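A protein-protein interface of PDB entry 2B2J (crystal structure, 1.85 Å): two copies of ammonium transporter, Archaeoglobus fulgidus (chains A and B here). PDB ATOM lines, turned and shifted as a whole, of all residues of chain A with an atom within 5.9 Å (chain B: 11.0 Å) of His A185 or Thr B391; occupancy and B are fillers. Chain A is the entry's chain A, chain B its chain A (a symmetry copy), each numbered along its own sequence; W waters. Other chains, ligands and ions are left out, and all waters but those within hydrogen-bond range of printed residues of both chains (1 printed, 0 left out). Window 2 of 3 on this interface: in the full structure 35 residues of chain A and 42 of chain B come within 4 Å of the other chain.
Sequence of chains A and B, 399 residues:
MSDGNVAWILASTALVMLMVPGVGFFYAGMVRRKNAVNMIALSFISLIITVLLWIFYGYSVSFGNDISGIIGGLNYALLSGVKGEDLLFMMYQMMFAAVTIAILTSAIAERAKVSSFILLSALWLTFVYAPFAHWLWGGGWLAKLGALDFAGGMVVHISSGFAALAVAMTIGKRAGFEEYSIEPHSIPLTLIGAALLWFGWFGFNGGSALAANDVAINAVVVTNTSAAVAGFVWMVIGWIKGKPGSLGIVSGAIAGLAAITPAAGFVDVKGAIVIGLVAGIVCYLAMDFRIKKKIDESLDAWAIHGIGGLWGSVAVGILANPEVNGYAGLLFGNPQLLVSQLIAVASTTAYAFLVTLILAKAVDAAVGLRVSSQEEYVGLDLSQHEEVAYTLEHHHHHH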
ATOM      1  N   ALA A  28      -1.657 -17.018  -8.250  1.00  0.00           N
ATOM      2  CA  ALA A  28      -2.764 -17.607  -7.493  1.00  0.00           C
ATOM      3  C   ALA A  28      -2.329 -18.600  -6.425  1.00  0.00           C
ATOM      4  O   ALA A  28      -2.866 -18.622  -5.312  1.00  0.00           O
ATOM      5  CB  ALA A  28      -3.733 -18.273  -8.437  1.00  0.00           C
ATOM      6  N   GLY A  29      -1.364 -19.440  -6.760  1.00  0.00           N
ATOM      7  CA  GLY A  29      -0.910 -20.416  -5.795  1.00  0.00           C
ATOM      8  C   GLY A  29      -0.275 -19.793  -4.569  1.00  0.00           C
ATOM      9  O   GLY A  29      -0.219 -20.429  -3.518  1.00  0.00           O
ATOM     10  N   MET A  30       0.196 -18.556  -4.688  1.00  0.00           N
ATOM     11  CA  MET A  30       0.851 -17.899  -3.572  1.00  0.00           C
ATOM     12  C   MET A  30      -0.083 -17.160  -2.633  1.00  0.00           C
ATOM     13  O   MET A  30       0.321 -16.782  -1.529  1.00  0.00           O
ATOM     14  CB  MET A  30       1.915 -16.947  -4.085  1.00  0.00           C
ATOM     15  CG  MET A  30       2.921 -17.648  -4.953  1.00  0.00           C
ATOM     16  SD  MET A  30       4.322 -16.630  -5.387  1.00  0.00           S
ATOM     17  CE  MET A  30       3.659 -15.665  -6.717  1.00  0.00           C
ATOM     18  N   VAL A  31      -1.323 -16.946  -3.063  1.00  0.00           N
ATOM     19  CA  VAL A  31      -2.294 -16.258  -2.222  1.00  0.00           C
ATOM     20  C   VAL A  31      -3.208 -17.271  -1.532  1.00  0.00           C
ATOM     21  O   VAL A  31      -3.213 -18.458  -1.871  1.00  0.00           O
ATOM     22  CB  VAL A  31      -3.160 -15.285  -3.046  1.00  0.00           C
ATOM     23  CG1 VAL A  31      -2.263 -14.364  -3.854  1.00  0.00           C
ATOM     24  CG2 VAL A  31      -4.109 -16.055  -3.949  1.00  0.00           C
ATOM     25  N   ARG A  32      -3.982 -16.800  -0.563  1.00  0.00           N
ATOM     26  CA  ARG A  32      -4.893 -17.668   0.163  1.00  0.00           C
ATOM     27  C   ARG A  32      -6.016 -18.224  -0.696  1.00  0.00           C
ATOM     28  O   ARG A  32      -6.423 -17.625  -1.690  1.00  0.00           O
ATOM     29  CB  ARG A  32      -5.465 -16.913   1.351  1.00  0.00           C
ATOM     30  CG  ARG A  32      -4.477 -16.796   2.490  1.00  0.00           C
ATOM     31  CD  ARG A  32      -4.889 -15.717   3.465  1.00  0.00           C
ATOM     32  NE  ARG A  32      -4.747 -14.395   2.864  1.00  0.00           N
ATOM     33  CZ  ARG A  32      -4.863 -13.254   3.537  1.00  0.00           C
ATOM     34  NH1 ARG A  32      -5.127 -13.280   4.836  1.00  0.00           N
ATOM     35  NH2 ARG A  32      -4.702 -12.090   2.919  1.00  0.00           N
ATOM     36  N   ARG A  33      -6.517 -19.382  -0.293  1.00  0.00           N
ATOM     37  CA  ARG A  33      -7.580 -20.060  -1.012  1.00  0.00           C
ATOM     38  C   ARG A  33      -8.775 -19.163  -1.310  1.00  0.00           C
ATOM     39  O   ARG A  33      -9.449 -19.335  -2.332  1.00  0.00           O
ATOM     40  CB  ARG A  33      -8.032 -21.280  -0.209  1.00  0.00           C
ATOM     41  CG  ARG A  33      -9.215 -22.018  -0.790  1.00  0.00           C
ATOM     42  CD  ARG A  33      -9.677 -23.112   0.165  1.00  0.00           C
ATOM     43  NE  ARG A  33     -10.942 -23.717  -0.252  1.00  0.00           N
ATOM     44  CZ  ARG A  33     -11.516 -24.738   0.377  1.00  0.00           C
ATOM     45  NH1 ARG A  33     -10.934 -25.265   1.448  1.00  0.00           N
ATOM     46  NH2 ARG A  33     -12.670 -25.230  -0.062  1.00  0.00           N
ATOM     47  N   ALA A  36      -7.942 -17.174  -4.582  1.00  0.00           N
ATOM     48  CA  ALA A  36      -7.403 -17.903  -5.715  1.00  0.00           C
ATOM     49  C   ALA A  36      -8.044 -17.505  -7.034  1.00  0.00           C
ATOM     50  O   ALA A  36      -7.345 -17.170  -7.987  1.00  0.00           O
ATOM     51  CB  ALA A  36      -7.555 -19.385  -5.489  1.00  0.00           C
ATOM     52  N   GLU A 183       0.265 -17.576   3.957  1.00  0.00           N
ATOM     53  CA  GLU A 183       0.740 -18.835   3.388  1.00  0.00           C
ATOM     54  C   GLU A 183       0.159 -19.176   2.012  1.00  0.00           C
ATOM     55  O   GLU A 183      -1.017 -18.945   1.750  1.00  0.00           O
ATOM     56  CB  GLU A 183       0.438 -19.985   4.354  1.00  0.00           C
ATOM     57  CG  GLU A 183       1.240 -19.950   5.647  1.00  0.00           C
ATOM     58  CD  GLU A 183       2.734 -19.936   5.396  1.00  0.00           C
ATOM     59  OE1 GLU A 183       3.210 -20.759   4.585  1.00  0.00           O
ATOM     60  OE2 GLU A 183       3.437 -19.106   6.011  1.00  0.00           O
ATOM     61  N   PRO A 184       0.990 -19.726   1.113  1.00  0.00           N
ATOM     62  CA  PRO A 184       0.502 -20.090  -0.221  1.00  0.00           C
ATOM     63  C   PRO A 184      -0.523 -21.208  -0.066  1.00  0.00           C
ATOM     64  O   PRO A 184      -0.305 -22.143   0.706  1.00  0.00           O
ATOM     65  CB  PRO A 184       1.765 -20.563  -0.934  1.00  0.00           C
ATOM     66  CG  PRO A 184       2.596 -21.123   0.186  1.00  0.00           C
ATOM     67  CD  PRO A 184       2.412 -20.078   1.267  1.00  0.00           C
ATOM     68  N   HIS A 185      -1.636 -21.125  -0.787  1.00  0.00           N
ATOM     69  CA  HIS A 185      -2.644 -22.162  -0.659  1.00  0.00           C
ATOM     70  C   HIS A 185      -2.371 -23.365  -1.553  1.00  0.00           C
ATOM     71  O   HIS A 185      -2.820 -24.470  -1.261  1.00  0.00           O
ATOM     72  CB  HIS A 185      -4.047 -21.605  -0.945  1.00  0.00           C
ATOM     73  CG  HIS A 185      -4.434 -21.619  -2.393  1.00  0.00           C
ATOM     74  ND1 HIS A 185      -4.122 -20.596  -3.262  1.00  0.00           N
ATOM     75  CD2 HIS A 185      -5.105 -22.545  -3.123  1.00  0.00           C
ATOM     76  CE1 HIS A 185      -4.581 -20.893  -4.467  1.00  0.00           C
ATOM     77  NE2 HIS A 185      -5.182 -22.069  -4.409  1.00  0.00           N
ATOM     78  N   SER A 186      -1.635 -23.166  -2.639  1.00  0.00           N
ATOM     79  CA  SER A 186      -1.348 -24.281  -3.530  1.00  0.00           C
ATOM     80  C   SER A 186      -0.055 -24.073  -4.281  1.00  0.00           C
ATOM     81  O   SER A 186      -0.034 -23.497  -5.370  1.00  0.00           O
ATOM     82  CB  SER A 186      -2.481 -24.463  -4.527  1.00  0.00           C
ATOM     83  OG  SER A 186      -2.131 -25.443  -5.480  1.00  0.00           O
ATOM     84  N   ILE A 187       1.036 -24.541  -3.694  1.00  0.00           N
ATOM     85  CA  ILE A 187       2.326 -24.388  -4.337  1.00  0.00           C
ATOM     86  C   ILE A 187       2.285 -25.084  -5.701  1.00  0.00           C
ATOM     87  O   ILE A 187       2.787 -24.548  -6.700  1.00  0.00           O
ATOM     88  CB  ILE A 187       3.448 -24.942  -3.430  1.00  0.00           C
ATOM     89  CG1 ILE A 187       3.551 -24.073  -2.167  1.00  0.00           C
ATOM     90  CG2 ILE A 187       4.772 -24.931  -4.161  1.00  0.00           C
ATOM     91  CD1 ILE A 187       4.705 -24.450  -1.200  1.00  0.00           C
ATOM     92  N   LEU A 189      -0.065 -25.326  -7.796  1.00  0.00           N
ATOM     93  CA  LEU A 189      -0.737 -24.454  -8.764  1.00  0.00           C
ATOM     94  C   LEU A 189       0.277 -23.427  -9.262  1.00  0.00           C
ATOM     95  O   LEU A 189       0.358 -23.125 -10.459  1.00  0.00           O
ATOM     96  CB  LEU A 189      -1.931 -23.740  -8.120  1.00  0.00           C
ATOM     97  CG  LEU A 189      -2.635 -22.738  -9.051  1.00  0.00           C
ATOM     98  CD1 LEU A 189      -3.098 -23.459 -10.319  1.00  0.00           C
ATOM     99  CD2 LEU A 189      -3.808 -22.083  -8.359  1.00  0.00           C
ATOM    100  N   TYR A 390     -12.576 -23.575  -4.370  1.00  0.00           N
ATOM    101  CA  TYR A 390     -12.722 -25.003  -4.200  1.00  0.00           C
ATOM    102  C   TYR A 390     -13.854 -25.377  -3.269  1.00  0.00           C
ATOM    103  O   TYR A 390     -14.229 -24.620  -2.377  1.00  0.00           O
ATOM    104  CB  TYR A 390     -11.440 -25.598  -3.638  1.00  0.00           C
ATOM    105  CG  TYR A 390     -10.181 -25.064  -4.260  1.00  0.00           C
ATOM    106  CD1 TYR A 390      -9.558 -23.927  -3.749  1.00  0.00           C
ATOM    107  CD2 TYR A 390      -9.599 -25.705  -5.351  1.00  0.00           C
ATOM    108  CE1 TYR A 390      -8.385 -23.448  -4.305  1.00  0.00           C
ATOM    109  CE2 TYR A 390      -8.425 -25.233  -5.918  1.00  0.00           C
ATOM    110  CZ  TYR A 390      -7.823 -24.110  -5.390  1.00  0.00           C
ATOM    111  OH  TYR A 390      -6.648 -23.667  -5.936  1.00  0.00           O
ATOM    112  N   ARG B  33       0.156 -36.151  -0.575  1.00  0.00           N
ATOM    113  CA  ARG B  33       0.125 -34.704  -0.461  1.00  0.00           C
ATOM    114  C   ARG B  33       1.361 -34.124   0.214  1.00  0.00           C
ATOM    115  O   ARG B  33       1.783 -33.007  -0.102  1.00  0.00           O
ATOM    116  CB  ARG B  33      -1.131 -34.288   0.305  1.00  0.00           C
ATOM    117  CG  ARG B  33      -1.235 -32.807   0.594  1.00  0.00           C
ATOM    118  CD  ARG B  33      -2.435 -32.527   1.491  1.00  0.00           C
ATOM    119  NE  ARG B  33      -2.460 -31.146   1.969  1.00  0.00           N
ATOM    120  CZ  ARG B  33      -3.441 -30.638   2.710  1.00  0.00           C
ATOM    121  NH1 ARG B  33      -4.473 -31.400   3.052  1.00  0.00           N
ATOM    122  NH2 ARG B  33      -3.390 -29.372   3.110  1.00  0.00           N
ATOM    123  N   LYS B  34       1.956 -34.882   1.130  1.00  0.00           N
ATOM    124  CA  LYS B  34       3.130 -34.397   1.860  1.00  0.00           C
ATOM    125  C   LYS B  34       4.426 -34.394   1.065  1.00  0.00           C
ATOM    126  O   LYS B  34       5.454 -33.913   1.555  1.00  0.00           O
ATOM    127  CB  LYS B  34       3.335 -35.214   3.136  1.00  0.00           C
ATOM    128  CG  LYS B  34       3.740 -36.651   2.903  1.00  0.00           C
ATOM    129  CD  LYS B  34       3.759 -37.401   4.220  1.00  0.00           C
ATOM    130  CE  LYS B  34       4.119 -38.860   4.021  1.00  0.00           C
ATOM    131  NZ  LYS B  34       3.920 -39.635   5.277  1.00  0.00           N
ATOM    132  N   ALA B  36       4.125 -33.764  -2.540  1.00  0.00           N
ATOM    133  CA  ALA B  36       3.761 -33.164  -3.810  1.00  0.00           C
ATOM    134  C   ALA B  36       4.789 -32.161  -4.308  1.00  0.00           C
ATOM    135  O   ALA B  36       5.250 -32.259  -5.442  1.00  0.00           O
ATOM    136  CB  ALA B  36       2.408 -32.509  -3.696  1.00  0.00           C
ATOM    137  N   VAL B  37       5.145 -31.194  -3.474  1.00  0.00           N
ATOM    138  CA  VAL B  37       6.113 -30.193  -3.889  1.00  0.00           C
ATOM    139  C   VAL B  37       7.430 -30.842  -4.265  1.00  0.00           C
ATOM    140  O   VAL B  37       8.054 -30.493  -5.263  1.00  0.00           O
ATOM    141  CB  VAL B  37       6.385 -29.174  -2.773  1.00  0.00           C
ATOM    142  CG1 VAL B  37       7.531 -28.258  -3.168  1.00  0.00           C
ATOM    143  CG2 VAL B  37       5.145 -28.357  -2.519  1.00  0.00           C
ATOM    144  N   HIS B 185      -2.549 -38.435  -4.392  1.00  0.00           N
ATOM    145  CA  HIS B 185      -3.234 -37.339  -3.731  1.00  0.00           C
ATOM    146  C   HIS B 185      -4.033 -36.473  -4.695  1.00  0.00           C
ATOM    147  O   HIS B 185      -4.996 -35.822  -4.295  1.00  0.00           O
ATOM    148  CB  HIS B 185      -2.245 -36.467  -2.941  1.00  0.00           C
ATOM    149  CG  HIS B 185      -1.602 -35.378  -3.747  1.00  0.00           C
ATOM    150  ND1 HIS B 185      -0.456 -35.572  -4.489  1.00  0.00           N
ATOM    151  CD2 HIS B 185      -1.957 -34.082  -3.930  1.00  0.00           C
ATOM    152  CE1 HIS B 185      -0.135 -34.442  -5.097  1.00  0.00           C
ATOM    153  NE2 HIS B 185      -1.029 -33.523  -4.774  1.00  0.00           N
ATOM    154  N   ASP B 381       8.244 -32.520   1.536  1.00  0.00           N
ATOM    155  CA  ASP B 381       7.924 -31.132   1.249  1.00  0.00           C
ATOM    156  C   ASP B 381       8.414 -30.338   2.446  1.00  0.00           C
ATOM    157  O   ASP B 381       9.158 -29.370   2.315  1.00  0.00           O
ATOM    158  CB  ASP B 381       6.422 -30.949   1.092  1.00  0.00           C
ATOM    159  CG  ASP B 381       5.906 -31.550  -0.185  1.00  0.00           C
ATOM    160  OD1 ASP B 381       6.699 -32.228  -0.879  1.00  0.00           O
ATOM    161  OD2 ASP B 381       4.711 -31.353  -0.498  1.00  0.00           O
ATOM    162  N   LEU B 382       8.008 -30.784   3.624  1.00  0.00           N
ATOM    163  CA  LEU B 382       8.387 -30.131   4.863  1.00  0.00           C
ATOM    164  C   LEU B 382       9.864 -30.317   5.203  1.00  0.00           C
ATOM    165  O   LEU B 382      10.580 -29.347   5.455  1.00  0.00           O
ATOM    166  CB  LEU B 382       7.547 -30.680   6.013  1.00  0.00           C
ATOM    167  CG  LEU B 382       7.148 -29.700   7.112  1.00  0.00           C
ATOM    168  CD1 LEU B 382       8.307 -28.784   7.458  1.00  0.00           C
ATOM    169  CD2 LEU B 382       5.991 -28.877   6.621  1.00  0.00           C
ATOM    170  N   GLU B 386      11.076 -27.456   3.400  1.00  0.00           N
ATOM    171  CA  GLU B 386      10.486 -26.595   4.406  1.00  0.00           C
ATOM    172  C   GLU B 386       9.278 -25.888   3.806  1.00  0.00           C
ATOM    173  O   GLU B 386       9.074 -24.694   4.030  1.00  0.00           O
ATOM    174  CB  GLU B 386      11.494 -25.560   4.897  1.00  0.00           C
ATOM    175  CG  GLU B 386      12.507 -26.104   5.880  1.00  0.00           C
ATOM    176  CD  GLU B 386      13.337 -25.003   6.516  1.00  0.00           C
ATOM    177  OE1 GLU B 386      14.187 -25.313   7.380  1.00  0.00           O
ATOM    178  OE2 GLU B 386      13.140 -23.825   6.149  1.00  0.00           O
ATOM    179  N   GLU B 387       8.490 -26.626   3.027  1.00  0.00           N
ATOM    180  CA  GLU B 387       7.290 -26.078   2.408  1.00  0.00           C
ATOM    181  C   GLU B 387       6.087 -26.985   2.629  1.00  0.00           C
ATOM    182  O   GLU B 387       6.216 -28.122   3.074  1.00  0.00           O
ATOM    183  CB  GLU B 387       7.504 -25.879   0.906  1.00  0.00           C
ATOM    184  CG  GLU B 387       8.171 -24.569   0.536  1.00  0.00           C
ATOM    185  CD  GLU B 387       8.562 -24.500  -0.930  1.00  0.00           C
ATOM    186  OE1 GLU B 387       8.807 -23.378  -1.420  1.00  0.00           O
ATOM    187  OE2 GLU B 387       8.637 -25.564  -1.586  1.00  0.00           O
ATOM    188  N   VAL B 388       4.911 -26.459   2.317  1.00  0.00           N
ATOM    189  CA  VAL B 388       3.672 -27.207   2.449  1.00  0.00           C
ATOM    190  C   VAL B 388       2.886 -27.013   1.164  1.00  0.00           C
ATOM    191  O   VAL B 388       2.535 -25.892   0.799  1.00  0.00           O
ATOM    192  CB  VAL B 388       2.849 -26.713   3.644  1.00  0.00           C
ATOM    193  CG1 VAL B 388       1.565 -27.515   3.769  1.00  0.00           C
ATOM    194  CG2 VAL B 388       3.671 -26.851   4.909  1.00  0.00           C
ATOM    195  N   ALA B 389       2.629 -28.120   0.479  1.00  0.00           N
ATOM    196  CA  ALA B 389       1.915 -28.110  -0.791  1.00  0.00           C
ATOM    197  C   ALA B 389       0.610 -27.324  -0.770  1.00  0.00           C
ATOM    198  O   ALA B 389       0.448 -26.339  -1.483  1.00  0.00           O
ATOM    199  CB  ALA B 389       1.655 -29.551  -1.234  1.00  0.00           C
ATOM    200  N   TYR B 390      -0.324 -27.768   0.055  1.00  0.00           N
ATOM    201  CA  TYR B 390      -1.609 -27.109   0.128  1.00  0.00           C
ATOM    202  C   TYR B 390      -1.977 -26.683   1.533  1.00  0.00           C
ATOM    203  O   TYR B 390      -1.542 -27.274   2.518  1.00  0.00           O
ATOM    204  CB  TYR B 390      -2.702 -28.036  -0.380  1.00  0.00           C
ATOM    205  CG  TYR B 390      -2.344 -28.797  -1.625  1.00  0.00           C
ATOM    206  CD1 TYR B 390      -1.706 -30.033  -1.549  1.00  0.00           C
ATOM    207  CD2 TYR B 390      -2.659 -28.288  -2.884  1.00  0.00           C
ATOM    208  CE1 TYR B 390      -1.399 -30.746  -2.694  1.00  0.00           C
ATOM    209  CE2 TYR B 390      -2.353 -28.993  -4.038  1.00  0.00           C
ATOM    210  CZ  TYR B 390      -1.728 -30.219  -3.936  1.00  0.00           C
ATOM    211  OH  TYR B 390      -1.456 -30.923  -5.079  1.00  0.00           O
ATOM    212  N   THR B 391      -2.811 -25.659   1.595  1.00  0.00           N
ATOM    213  CA  THR B 391      -3.312 -25.114   2.838  1.00  0.00           C
ATOM    214  C   THR B 391      -4.806 -24.890   2.629  1.00  0.00           C
ATOM    215  O   THR B 391      -5.151 -23.760   2.222  1.00  0.00           O
ATOM    216  CB  THR B 391      -2.622 -23.780   3.167  1.00  0.00           C
ATOM    217  OG1 THR B 391      -1.226 -24.016   3.405  1.00  0.00           O
ATOM    218  CG2 THR B 391      -3.242 -23.144   4.398  1.00  0.00           C
HETATM  219  O   HOH W   1      -5.540 -20.613   2.244  1.00  0.00           O
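His A185 touches Tyr B390, but with the chains exchanged Tyr A390 does not touch His B185 (11.1 Å).
Positions printed for both chains: 33, 36, 185 and 390.
Of the 10 pairs that touch across the chains among the printed residues, none has its exchanged pair printed and touching as well.
Among the printed residues, pairs that only touch across the chains: His A185 with Ala B389, His A185 with Tyr B390, Ser A186 with Ala B389, Ser A186 with Tyr B390, Ile A187 with Val B37, Ile A187 with Glu B387 and Ile A187 with Val B388.
His A185 touches three residues of chain B.
Of chain A, only Pro A184 and His A185 come within 4 Å of Thr B391.
No residue of chain B comes within 4 Å of Ala A28.
No residue of chain B comes within 4 Å of Gly A29.
No residue of chain B comes within 4 Å of Val A31.
No residue of chain B comes within 4 Å of Ala A36.
Of chain B, only Thr B391 comes within 4 Å of Pro A184.
Printed residues of chain B within 4 Å of Ile A187: Val B37, Glu B387, Val B388 and Ala B389.
Printed residues of chain A within 4 Å of Ala B389: His A185 (3.8 Å), Ser A186 (3.4 Å) and Ile A187 (2.9 Å).
Of the printed residues of chain A, Glu B387 touches Ile A187.
Printed residues of chain A within 4 Å of Tyr B390: His A185 and Ser A186.
Arg A33 touches none of the printed residues of chain B.
Ala B36 touches none of the printed residues of chain A.
The nearest residue of chain B that does not touch His A185 is Val B388 (5.9 Å).
N of Val B37 lies within hydrogen-bond range of OD2 of Asp B381 (3.0 Å).
The side-chain hydroxyl of Tyr A390 lies within hydrogen-bond range of a ring nitrogen (NE2) of His A185 (2.7 Å).
O of Asp B381 lies within hydrogen-bond range of N of Glu B387, 2.9 Å away.
ND1 of His A185 sits close to O of Ala A28, at 3.1 Å.
The backbone NH (N) of Leu B382 lies within hydrogen-bond range of the backbone carbonyl oxygen (O) of Glu B387.
A ring nitrogen (NE2) of His B185 is in hydrogen-bond range of the side-chain hydroxyl of Tyr B390 (2.7 Å).
Water W1 bridges N of Arg A33 (3.0 Å) and O of Thr B391 (3.2 Å).
Of the 14 printed residues of chain A, 4 touch a printed residue of chain B.
Printed residues of chain A that touch a printed residue of chain B: Pro A184, His A185, Ser A186 and Ile A187.
Among the printed residues, no Asp or Glu carboxylate lies within 4 Å of a Lys or Arg side-chain nitrogen of the other chain.
The side-chain hydroxyl (OG1) of Thr B391 lies within hydrogen-bond range of the backbone carbonyl oxygen (O) of Pro A184.
N of Ile A187 lies within hydrogen-bond range of O of Ala B389, 2.9 Å away.
The backbone carbonyl oxygen of His A185 sits at hydrogen-bond distance from the backbone NH of Thr B391, 3.1 Å away.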
